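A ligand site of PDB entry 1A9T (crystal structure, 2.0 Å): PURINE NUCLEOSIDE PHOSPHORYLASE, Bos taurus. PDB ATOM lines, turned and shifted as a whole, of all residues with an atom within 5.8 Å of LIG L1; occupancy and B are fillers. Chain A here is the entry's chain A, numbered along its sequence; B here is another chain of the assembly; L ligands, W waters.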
ATOM      1  N   CYS A  31     -26.904 -15.230 -11.968  1.00  0.00           N
ATOM      2  CA  CYS A  31     -26.135 -16.423 -12.298  1.00  0.00           C
ATOM      3  C   CYS A  31     -24.660 -16.132 -12.585  1.00  0.00           C
ATOM      4  O   CYS A  31     -24.325 -15.256 -13.397  1.00  0.00           O
ATOM      5  CB  CYS A  31     -26.756 -17.143 -13.491  1.00  0.00           C
ATOM      6  SG  CYS A  31     -28.527 -17.522 -13.326  1.00  0.00           S
ATOM      7  N   GLY A  32     -23.789 -16.883 -11.907  1.00  0.00           N
ATOM      8  CA  GLY A  32     -22.368 -16.706 -12.090  1.00  0.00           C
ATOM      9  C   GLY A  32     -21.787 -17.573 -13.193  1.00  0.00           C
ATOM     10  O   GLY A  32     -22.515 -18.132 -14.008  1.00  0.00           O
ATOM     11  N   SER A  33     -20.450 -17.689 -13.188  1.00  0.00           N
ATOM     12  CA  SER A  33     -19.730 -18.470 -14.187  1.00  0.00           C
ATOM     13  C   SER A  33     -20.176 -19.924 -14.233  1.00  0.00           C
ATOM     14  O   SER A  33     -20.201 -20.606 -13.195  1.00  0.00           O
ATOM     15  CB  SER A  33     -18.223 -18.408 -13.937  1.00  0.00           C
ATOM     16  OG  SER A  33     -17.709 -17.117 -14.186  1.00  0.00           O
ATOM     17  N   LEU A  35     -23.034 -21.083 -14.472  1.00  0.00           N
ATOM     18  CA  LEU A  35     -24.302 -21.302 -13.774  1.00  0.00           C
ATOM     19  C   LEU A  35     -25.489 -20.799 -14.604  1.00  0.00           C
ATOM     20  O   LEU A  35     -26.633 -20.825 -14.161  1.00  0.00           O
ATOM     21  CB  LEU A  35     -24.291 -20.620 -12.408  1.00  0.00           C
ATOM     22  CG  LEU A  35     -23.078 -20.946 -11.516  1.00  0.00           C
ATOM     23  CD1 LEU A  35     -23.231 -20.264 -10.182  1.00  0.00           C
ATOM     24  CD2 LEU A  35     -22.918 -22.455 -11.343  1.00  0.00           C
ATOM     25  N   VAL A  61     -17.408 -11.553 -20.253  1.00  0.00           N
ATOM     26  CA  VAL A  61     -16.714 -12.758 -19.819  1.00  0.00           C
ATOM     27  C   VAL A  61     -17.338 -14.064 -20.288  1.00  0.00           C
ATOM     28  O   VAL A  61     -18.538 -14.296 -20.094  1.00  0.00           O
ATOM     29  CB  VAL A  61     -16.587 -12.780 -18.273  1.00  0.00           C
ATOM     30  CG1 VAL A  61     -15.947 -14.086 -17.787  1.00  0.00           C
ATOM     31  CG2 VAL A  61     -15.781 -11.570 -17.803  1.00  0.00           C
ATOM     32  N   HIS A  64     -20.815 -16.005 -19.443  1.00  0.00           N
ATOM     33  CA  HIS A  64     -21.806 -15.006 -19.089  1.00  0.00           C
ATOM     34  C   HIS A  64     -22.465 -14.538 -20.389  1.00  0.00           C
ATOM     35  O   HIS A  64     -21.914 -13.728 -21.117  1.00  0.00           O
ATOM     36  CB  HIS A  64     -21.155 -13.837 -18.352  1.00  0.00           C
ATOM     37  CG  HIS A  64     -20.546 -14.220 -17.031  1.00  0.00           C
ATOM     38  ND1 HIS A  64     -19.337 -14.864 -16.923  1.00  0.00           N
ATOM     39  CD2 HIS A  64     -21.007 -14.068 -15.768  1.00  0.00           C
ATOM     40  CE1 HIS A  64     -19.076 -15.098 -15.649  1.00  0.00           C
ATOM     41  NE2 HIS A  64     -20.075 -14.632 -14.933  1.00  0.00           N
ATOM     42  N   ARG A  84     -23.158 -11.909 -15.239  1.00  0.00           N
ATOM     43  CA  ARG A  84     -23.069 -10.695 -14.443  1.00  0.00           C
ATOM     44  C   ARG A  84     -21.870  -9.858 -14.848  1.00  0.00           C
ATOM     45  O   ARG A  84     -21.191 -10.176 -15.822  1.00  0.00           O
ATOM     46  CB  ARG A  84     -22.976 -11.047 -12.953  1.00  0.00           C
ATOM     47  CG  ARG A  84     -21.795 -11.918 -12.580  1.00  0.00           C
ATOM     48  CD  ARG A  84     -21.187 -11.507 -11.259  1.00  0.00           C
ATOM     49  NE  ARG A  84     -22.097 -11.662 -10.124  1.00  0.00           N
ATOM     50  CZ  ARG A  84     -22.340 -12.814  -9.510  1.00  0.00           C
ATOM     51  NH1 ARG A  84     -21.752 -13.939  -9.924  1.00  0.00           N
ATOM     52  NH2 ARG A  84     -23.140 -12.840  -8.441  1.00  0.00           N
ATOM     53  N   HIS A  86     -18.233  -7.706 -13.548  1.00  0.00           N
ATOM     54  CA  HIS A  86     -17.157  -7.773 -12.567  1.00  0.00           C
ATOM     55  C   HIS A  86     -16.315  -6.516 -12.688  1.00  0.00           C
ATOM     56  O   HIS A  86     -16.236  -5.929 -13.767  1.00  0.00           O
ATOM     57  CB  HIS A  86     -16.277  -8.995 -12.829  1.00  0.00           C
ATOM     58  CG  HIS A  86     -17.028 -10.267 -13.025  1.00  0.00           C
ATOM     59  ND1 HIS A  86     -17.671 -10.590 -14.204  1.00  0.00           N
ATOM     60  CD2 HIS A  86     -17.197 -11.340 -12.213  1.00  0.00           C
ATOM     61  CE1 HIS A  86     -18.199 -11.801 -14.110  1.00  0.00           C
ATOM     62  NE2 HIS A  86     -17.923 -12.274 -12.902  1.00  0.00           N
ATOM     63  N   TYR A  88     -13.081  -6.392 -12.684  1.00  0.00           N
ATOM     64  CA  TYR A  88     -11.898  -6.643 -13.521  1.00  0.00           C
ATOM     65  C   TYR A  88     -12.135  -6.399 -15.020  1.00  0.00           C
ATOM     66  O   TYR A  88     -11.182  -6.408 -15.796  1.00  0.00           O
ATOM     67  CB  TYR A  88     -11.315  -8.041 -13.290  1.00  0.00           C
ATOM     68  CG  TYR A  88     -12.200  -9.202 -13.714  1.00  0.00           C
ATOM     69  CD1 TYR A  88     -12.466  -9.459 -15.059  1.00  0.00           C
ATOM     70  CD2 TYR A  88     -12.780 -10.032 -12.752  1.00  0.00           C
ATOM     71  CE1 TYR A  88     -13.301 -10.499 -15.441  1.00  0.00           C
ATOM     72  CE2 TYR A  88     -13.609 -11.073 -13.122  1.00  0.00           C
ATOM     73  CZ  TYR A  88     -13.868 -11.302 -14.466  1.00  0.00           C
ATOM     74  OH  TYR A  88     -14.747 -12.301 -14.813  1.00  0.00           O
ATOM     75  N   THR A 114     -25.407 -16.122  -6.894  1.00  0.00           N
ATOM     76  CA  THR A 114     -24.622 -17.355  -7.007  1.00  0.00           C
ATOM     77  C   THR A 114     -23.295 -17.018  -7.660  1.00  0.00           C
ATOM     78  O   THR A 114     -23.157 -15.983  -8.312  1.00  0.00           O
ATOM     79  CB  THR A 114     -25.323 -18.404  -7.893  1.00  0.00           C
ATOM     80  OG1 THR A 114     -25.378 -17.942  -9.250  1.00  0.00           O
ATOM     81  CG2 THR A 114     -26.753 -18.681  -7.402  1.00  0.00           C
ATOM     82  N   ASN A 115     -22.325 -17.893  -7.501  1.00  0.00           N
ATOM     83  CA  ASN A 115     -21.021 -17.675  -8.113  1.00  0.00           C
ATOM     84  C   ASN A 115     -20.216 -18.958  -8.069  1.00  0.00           C
ATOM     85  O   ASN A 115     -20.623 -19.936  -7.444  1.00  0.00           O
ATOM     86  CB  ASN A 115     -20.262 -16.543  -7.402  1.00  0.00           C
ATOM     87  CG  ASN A 115     -19.976 -16.850  -5.937  1.00  0.00           C
ATOM     88  OD1 ASN A 115     -19.345 -17.850  -5.607  1.00  0.00           O
ATOM     89  ND2 ASN A 115     -20.427 -15.968  -5.045  1.00  0.00           N
ATOM     90  N   ALA A 116     -19.121 -18.963  -8.811  1.00  0.00           N
ATOM     91  CA  ALA A 116     -18.205 -20.076  -8.867  1.00  0.00           C
ATOM     92  C   ALA A 116     -17.065 -19.538  -8.002  1.00  0.00           C
ATOM     93  O   ALA A 116     -16.690 -18.379  -8.164  1.00  0.00           O
ATOM     94  CB  ALA A 116     -17.728 -20.300 -10.300  1.00  0.00           C
ATOM     95  N   ALA A 117     -16.566 -20.337  -7.063  1.00  0.00           N
ATOM     96  CA  ALA A 117     -15.496 -19.864  -6.196  1.00  0.00           C
ATOM     97  C   ALA A 117     -14.424 -20.919  -5.995  1.00  0.00           C
ATOM     98  O   ALA A 117     -14.670 -22.111  -6.148  1.00  0.00           O
ATOM     99  CB  ALA A 117     -16.047 -19.434  -4.840  1.00  0.00           C
ATOM    100  N   TYR A 192     -17.290 -16.010   2.300  1.00  0.00           N
ATOM    101  CA  TYR A 192     -16.802 -15.775   0.962  1.00  0.00           C
ATOM    102  C   TYR A 192     -15.923 -14.521   0.989  1.00  0.00           C
ATOM    103  O   TYR A 192     -16.295 -13.517   1.605  1.00  0.00           O
ATOM    104  CB  TYR A 192     -17.998 -15.576   0.019  1.00  0.00           C
ATOM    105  CG  TYR A 192     -17.664 -15.188  -1.388  1.00  0.00           C
ATOM    106  CD1 TYR A 192     -17.552 -13.845  -1.759  1.00  0.00           C
ATOM    107  CD2 TYR A 192     -17.485 -16.154  -2.373  1.00  0.00           C
ATOM    108  CE1 TYR A 192     -17.281 -13.475  -3.059  1.00  0.00           C
ATOM    109  CE2 TYR A 192     -17.219 -15.792  -3.695  1.00  0.00           C
ATOM    110  CZ  TYR A 192     -17.122 -14.457  -4.029  1.00  0.00           C
ATOM    111  OH  TYR A 192     -16.889 -14.098  -5.319  1.00  0.00           O
ATOM    112  N   PHE A 200      -5.379 -15.298 -11.121  1.00  0.00           N
ATOM    113  CA  PHE A 200      -5.643 -16.220 -10.042  1.00  0.00           C
ATOM    114  C   PHE A 200      -4.555 -16.004  -8.977  1.00  0.00           C
ATOM    115  O   PHE A 200      -3.498 -15.455  -9.276  1.00  0.00           O
ATOM    116  CB  PHE A 200      -5.709 -17.665 -10.534  1.00  0.00           C
ATOM    117  CG  PHE A 200      -6.987 -17.986 -11.276  1.00  0.00           C
ATOM    118  CD1 PHE A 200      -8.218 -17.883 -10.636  1.00  0.00           C
ATOM    119  CD2 PHE A 200      -6.961 -18.421 -12.591  1.00  0.00           C
ATOM    120  CE1 PHE A 200      -9.400 -18.190 -11.295  1.00  0.00           C
ATOM    121  CE2 PHE A 200      -8.134 -18.740 -13.257  1.00  0.00           C
ATOM    122  CZ  PHE A 200      -9.362 -18.627 -12.617  1.00  0.00           C
ATOM    123  N   GLY A 218     -13.446 -15.441  -4.507  1.00  0.00           N
ATOM    124  CA  GLY A 218     -14.047 -15.143  -5.790  1.00  0.00           C
ATOM    125  C   GLY A 218     -13.860 -13.674  -6.154  1.00  0.00           C
ATOM    126  O   GLY A 218     -13.338 -12.909  -5.343  1.00  0.00           O
ATOM    127  N   MET A 219     -14.331 -13.288  -7.336  1.00  0.00           N
ATOM    128  CA  MET A 219     -14.169 -11.913  -7.830  1.00  0.00           C
ATOM    129  C   MET A 219     -15.484 -11.166  -8.093  1.00  0.00           C
ATOM    130  O   MET A 219     -15.568 -10.337  -9.016  1.00  0.00           O
ATOM    131  CB  MET A 219     -13.347 -11.938  -9.131  1.00  0.00           C
ATOM    132  CG  MET A 219     -12.047 -12.727  -9.050  1.00  0.00           C
ATOM    133  SD  MET A 219     -11.317 -13.070 -10.679  1.00  0.00           S
ATOM    134  CE  MET A 219      -9.898 -14.064 -10.233  1.00  0.00           C
ATOM    135  N   SER A 220     -16.514 -11.427  -7.296  1.00  0.00           N
ATOM    136  CA  SER A 220     -17.797 -10.762  -7.492  1.00  0.00           C
ATOM    137  C   SER A 220     -18.687 -10.894  -6.268  1.00  0.00           C
ATOM    138  O   SER A 220     -18.199 -11.035  -5.146  1.00  0.00           O
ATOM    139  CB  SER A 220     -18.508 -11.398  -8.677  1.00  0.00           C
ATOM    140  OG  SER A 220     -18.987 -12.681  -8.300  1.00  0.00           O
ATOM    141  N   THR A 221     -19.991 -10.770  -6.494  1.00  0.00           N
ATOM    142  CA  THR A 221     -21.011 -10.946  -5.467  1.00  0.00           C
ATOM    143  C   THR A 221     -21.160  -9.929  -4.338  1.00  0.00           C
ATOM    144  O   THR A 221     -22.230  -9.348  -4.167  1.00  0.00           O
ATOM    145  CB  THR A 221     -20.922 -12.375  -4.890  1.00  0.00           C
ATOM    146  OG1 THR A 221     -21.052 -13.313  -5.965  1.00  0.00           O
ATOM    147  CG2 THR A 221     -22.036 -12.641  -3.877  1.00  0.00           C
ATOM    148  N   THR A 242     -15.655 -24.725  -7.547  1.00  0.00           N
ATOM    149  CA  THR A 242     -15.179 -25.262  -8.828  1.00  0.00           C
ATOM    150  C   THR A 242     -13.777 -25.848  -8.829  1.00  0.00           C
ATOM    151  O   THR A 242     -13.420 -26.624  -9.714  1.00  0.00           O
ATOM    152  CB  THR A 242     -15.248 -24.204  -9.947  1.00  0.00           C
ATOM    153  OG1 THR A 242     -14.518 -23.025  -9.564  1.00  0.00           O
ATOM    154  CG2 THR A 242     -16.696 -23.836 -10.233  1.00  0.00           C
ATOM    155  N   ASN A 256      -7.649 -22.411 -13.832  1.00  0.00           N
ATOM    156  CA  ASN A 256      -7.929 -21.975 -15.187  1.00  0.00           C
ATOM    157  C   ASN A 256      -9.441 -21.811 -15.346  1.00  0.00           C
ATOM    158  O   ASN A 256     -10.208 -22.544 -14.723  1.00  0.00           O
ATOM    159  CB  ASN A 256      -7.388 -22.978 -16.211  1.00  0.00           C
ATOM    160  CG  ASN A 256      -8.071 -24.326 -16.118  1.00  0.00           C
ATOM    161  OD1 ASN A 256      -9.007 -24.609 -16.878  1.00  0.00           O
ATOM    162  ND2 ASN A 256      -7.617 -25.165 -15.202  1.00  0.00           N
ATOM    163  N   HIS A 257      -9.853 -20.861 -16.170  1.00  0.00           N
ATOM    164  CA  HIS A 257     -11.264 -20.566 -16.399  1.00  0.00           C
ATOM    165  C   HIS A 257     -12.126 -21.697 -16.964  1.00  0.00           C
ATOM    166  O   HIS A 257     -13.287 -21.831 -16.584  1.00  0.00           O
ATOM    167  CB  HIS A 257     -11.404 -19.322 -17.288  1.00  0.00           C
ATOM    168  CG  HIS A 257     -12.782 -18.741 -17.331  1.00  0.00           C
ATOM    169  ND1 HIS A 257     -13.526 -18.504 -16.195  1.00  0.00           N
ATOM    170  CD2 HIS A 257     -13.555 -18.345 -18.380  1.00  0.00           C
ATOM    171  CE1 HIS A 257     -14.695 -17.967 -16.537  1.00  0.00           C
ATOM    172  NE2 HIS A 257     -14.725 -17.862 -17.856  1.00  0.00           N
ATOM    173  N   VAL A 260     -13.372 -24.170 -14.342  1.00  0.00           N
ATOM    174  CA  VAL A 260     -14.503 -23.683 -13.543  1.00  0.00           C
ATOM    175  C   VAL A 260     -15.805 -23.823 -14.333  1.00  0.00           C
ATOM    176  O   VAL A 260     -16.831 -24.232 -13.790  1.00  0.00           O
ATOM    177  CB  VAL A 260     -14.314 -22.229 -13.022  1.00  0.00           C
ATOM    178  CG1 VAL A 260     -12.848 -21.964 -12.690  1.00  0.00           C
ATOM    179  CG2 VAL A 260     -14.896 -21.213 -13.968  1.00  0.00           C
ATOM    180  N   PHE B 159      -7.849 -15.069 -17.788  1.00  0.00           N
ATOM    181  CA  PHE B 159      -7.585 -15.451 -16.410  1.00  0.00           C
ATOM    182  C   PHE B 159      -6.252 -16.188 -16.257  1.00  0.00           C
ATOM    183  O   PHE B 159      -6.226 -17.414 -16.142  1.00  0.00           O
ATOM    184  CB  PHE B 159      -8.695 -16.354 -15.867  1.00  0.00           C
ATOM    185  CG  PHE B 159     -10.066 -15.734 -15.900  1.00  0.00           C
ATOM    186  CD1 PHE B 159     -10.457 -14.818 -14.938  1.00  0.00           C
ATOM    187  CD2 PHE B 159     -10.964 -16.092 -16.896  1.00  0.00           C
ATOM    188  CE1 PHE B 159     -11.728 -14.254 -14.957  1.00  0.00           C
ATOM    189  CE2 PHE B 159     -12.234 -15.538 -16.924  1.00  0.00           C
ATOM    190  CZ  PHE B 159     -12.616 -14.614 -15.950  1.00  0.00           C
HETATM  191  C1  LIG L   1     -12.894 -17.658 -12.544  1.00  0.00           C
HETATM  192  O1  LIG L   1     -12.983 -18.934 -13.325  1.00  0.00           O
HETATM  193  C2  LIG L   1     -13.970 -16.637 -12.566  1.00  0.00           C
HETATM  194  O2  LIG L   1     -15.180 -17.351 -12.002  1.00  0.00           O
HETATM  195  C3  LIG L   1     -15.888 -16.678 -10.962  1.00  0.00           C
HETATM  196  C4  LIG L   1     -14.747 -15.603 -10.525  1.00  0.00           C
HETATM  197  O3  LIG L   1     -15.316 -14.437  -9.907  1.00  0.00           O
HETATM  198  C5  LIG L   1     -13.893 -15.286 -11.792  1.00  0.00           C
HETATM  199  O4  LIG L   1     -14.516 -14.204 -12.502  1.00  0.00           O
HETATM  200  O5  LIG L   1     -17.005 -15.669 -11.711  1.00  0.00           O
HETATM  201  P1  LIG L   1     -18.496 -15.309 -10.906  1.00  0.00           P
HETATM  202  O6  LIG L   1     -19.416 -14.399 -11.703  1.00  0.00           O
HETATM  203  O7  LIG L   1     -18.883 -16.754 -10.734  1.00  0.00           O
HETATM  204  O8  LIG L   1     -18.071 -14.834  -9.543  1.00  0.00           O
HETATM  205  N1  LG2 L   2      -9.849 -17.841  -7.493  1.00  0.00           N
HETATM  206  C1  LG2 L   2     -10.641 -16.726  -7.544  1.00  0.00           C
HETATM  207  N2  LG2 L   2     -11.894 -16.772  -8.019  1.00  0.00           N
HETATM  208  C2  LG2 L   2     -12.273 -18.048  -8.420  1.00  0.00           C
HETATM  209  C3  LG2 L   2     -11.524 -19.194  -8.392  1.00  0.00           C
HETATM  210  C4  LG2 L   2     -10.204 -19.154  -7.895  1.00  0.00           C
HETATM  211  O1  LG2 L   2      -9.419 -20.115  -7.802  1.00  0.00           O
HETATM  212  N3  LG2 L   2     -12.240 -20.250  -8.882  1.00  0.00           N
HETATM  213  C5  LG2 L   2     -13.459 -19.731  -9.218  1.00  0.00           C
HETATM  214  N4  LG2 L   2     -13.522 -18.393  -8.941  1.00  0.00           N
HETATM  215  O   HOH W   1     -16.792 -15.614  -7.322  1.00  0.00           O
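OH of Tyr 88 sits at hydrogen-bond distance from O4 of LIG L1 (3.0 Å). The backbone NH of Ser 33 is in hydrogen-bond range of an oxygen (O7) of LIG L1, at 3.1 Å. The backbone NH (N) of Met 219 lies within hydrogen-bond range of an oxygen (O3) of LIG L1 (3.0 Å). An oxygen (O8) of LIG L1 sits at hydrogen-bond distance from the side-chain hydroxyl (OG) of Ser 220 (2.6 Å). An oxygen (O5) of LIG L1 sits at hydrogen-bond distance from the side-chain hydroxyl (OG) of Ser 33, at 3.0 Å. NE2 of His 64 sits at hydrogen-bond distance from O6 of LIG L1, 3.3 Å away. NE2 of His 86 is in hydrogen-bond range of O6 of LIG L1, at 2.9 Å. O of Ala 116 sits close to N4 of LG2 L2, 3.3 Å away. NH1 of Arg 84 lies within salt-bridge range of O6 of LIG L1, at 3.0 Å. ND1 of His 257 is in hydrogen-bond range of O1 of LIG L1 (3.0 Å). The backbone NH (N) of Ala 116 lies within hydrogen-bond range of an oxygen (O7) of LIG L1 (2.9 Å).
Water W1 lies within hydrogen-bond range of OH of Tyr 192 (2.5 Å), O8 of LIG L1 (2.7 Å), O of Ala 116 (2.9 Å) and N of Met 219 (3.4 Å).
A ring nitrogen (ND1) of His 64 lies close to the backbone carbonyl oxygen (O) of Val 61, 3.3 Å away. The side-chain amide nitrogen (ND2) of Asn 115 is in hydrogen-bond range of the side-chain hydroxyl (OG1) of Thr 221 (2.9 Å). The guanidinium group of Arg 84 is in hydrogen-bond range of the backbone carbonyl oxygen of Thr 114, at 3.0 Å. The side-chain hydroxyl of Ser 220 sits at hydrogen-bond distance from the side-chain hydroxyl of Thr 221 (3.2 Å). NH1 of Arg 84 is in hydrogen-bond range of OG of Ser 220. The backbone NH (N) of Gly 32 sits at hydrogen-bond distance from the side-chain hydroxyl (OG1) of Thr 114 (3.3 Å). The backbone NH of Met 219 is in hydrogen-bond range of the side-chain hydroxyl of Tyr 192, 3.4 Å away. The guanidinium group (NH2) of Arg 84 lies within hydrogen-bond range of the side-chain hydroxyl (OG1) of Thr 221 (3.3 Å).
Merely in contact with LIG L1: Val 260 (3.0 Å), Asn 115 (3.5 Å), Phe 200 (3.7 Å), Phe 159 of chain B (3.7 Å) and Gly 32 (3.7 Å). Hydrophobic or aromatic side chains within 4 Å of LIG L1: His 86, Tyr 88, Ala 116, Phe 200, Met 219, His 257, Val 260 and Phe 159 of chain B.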
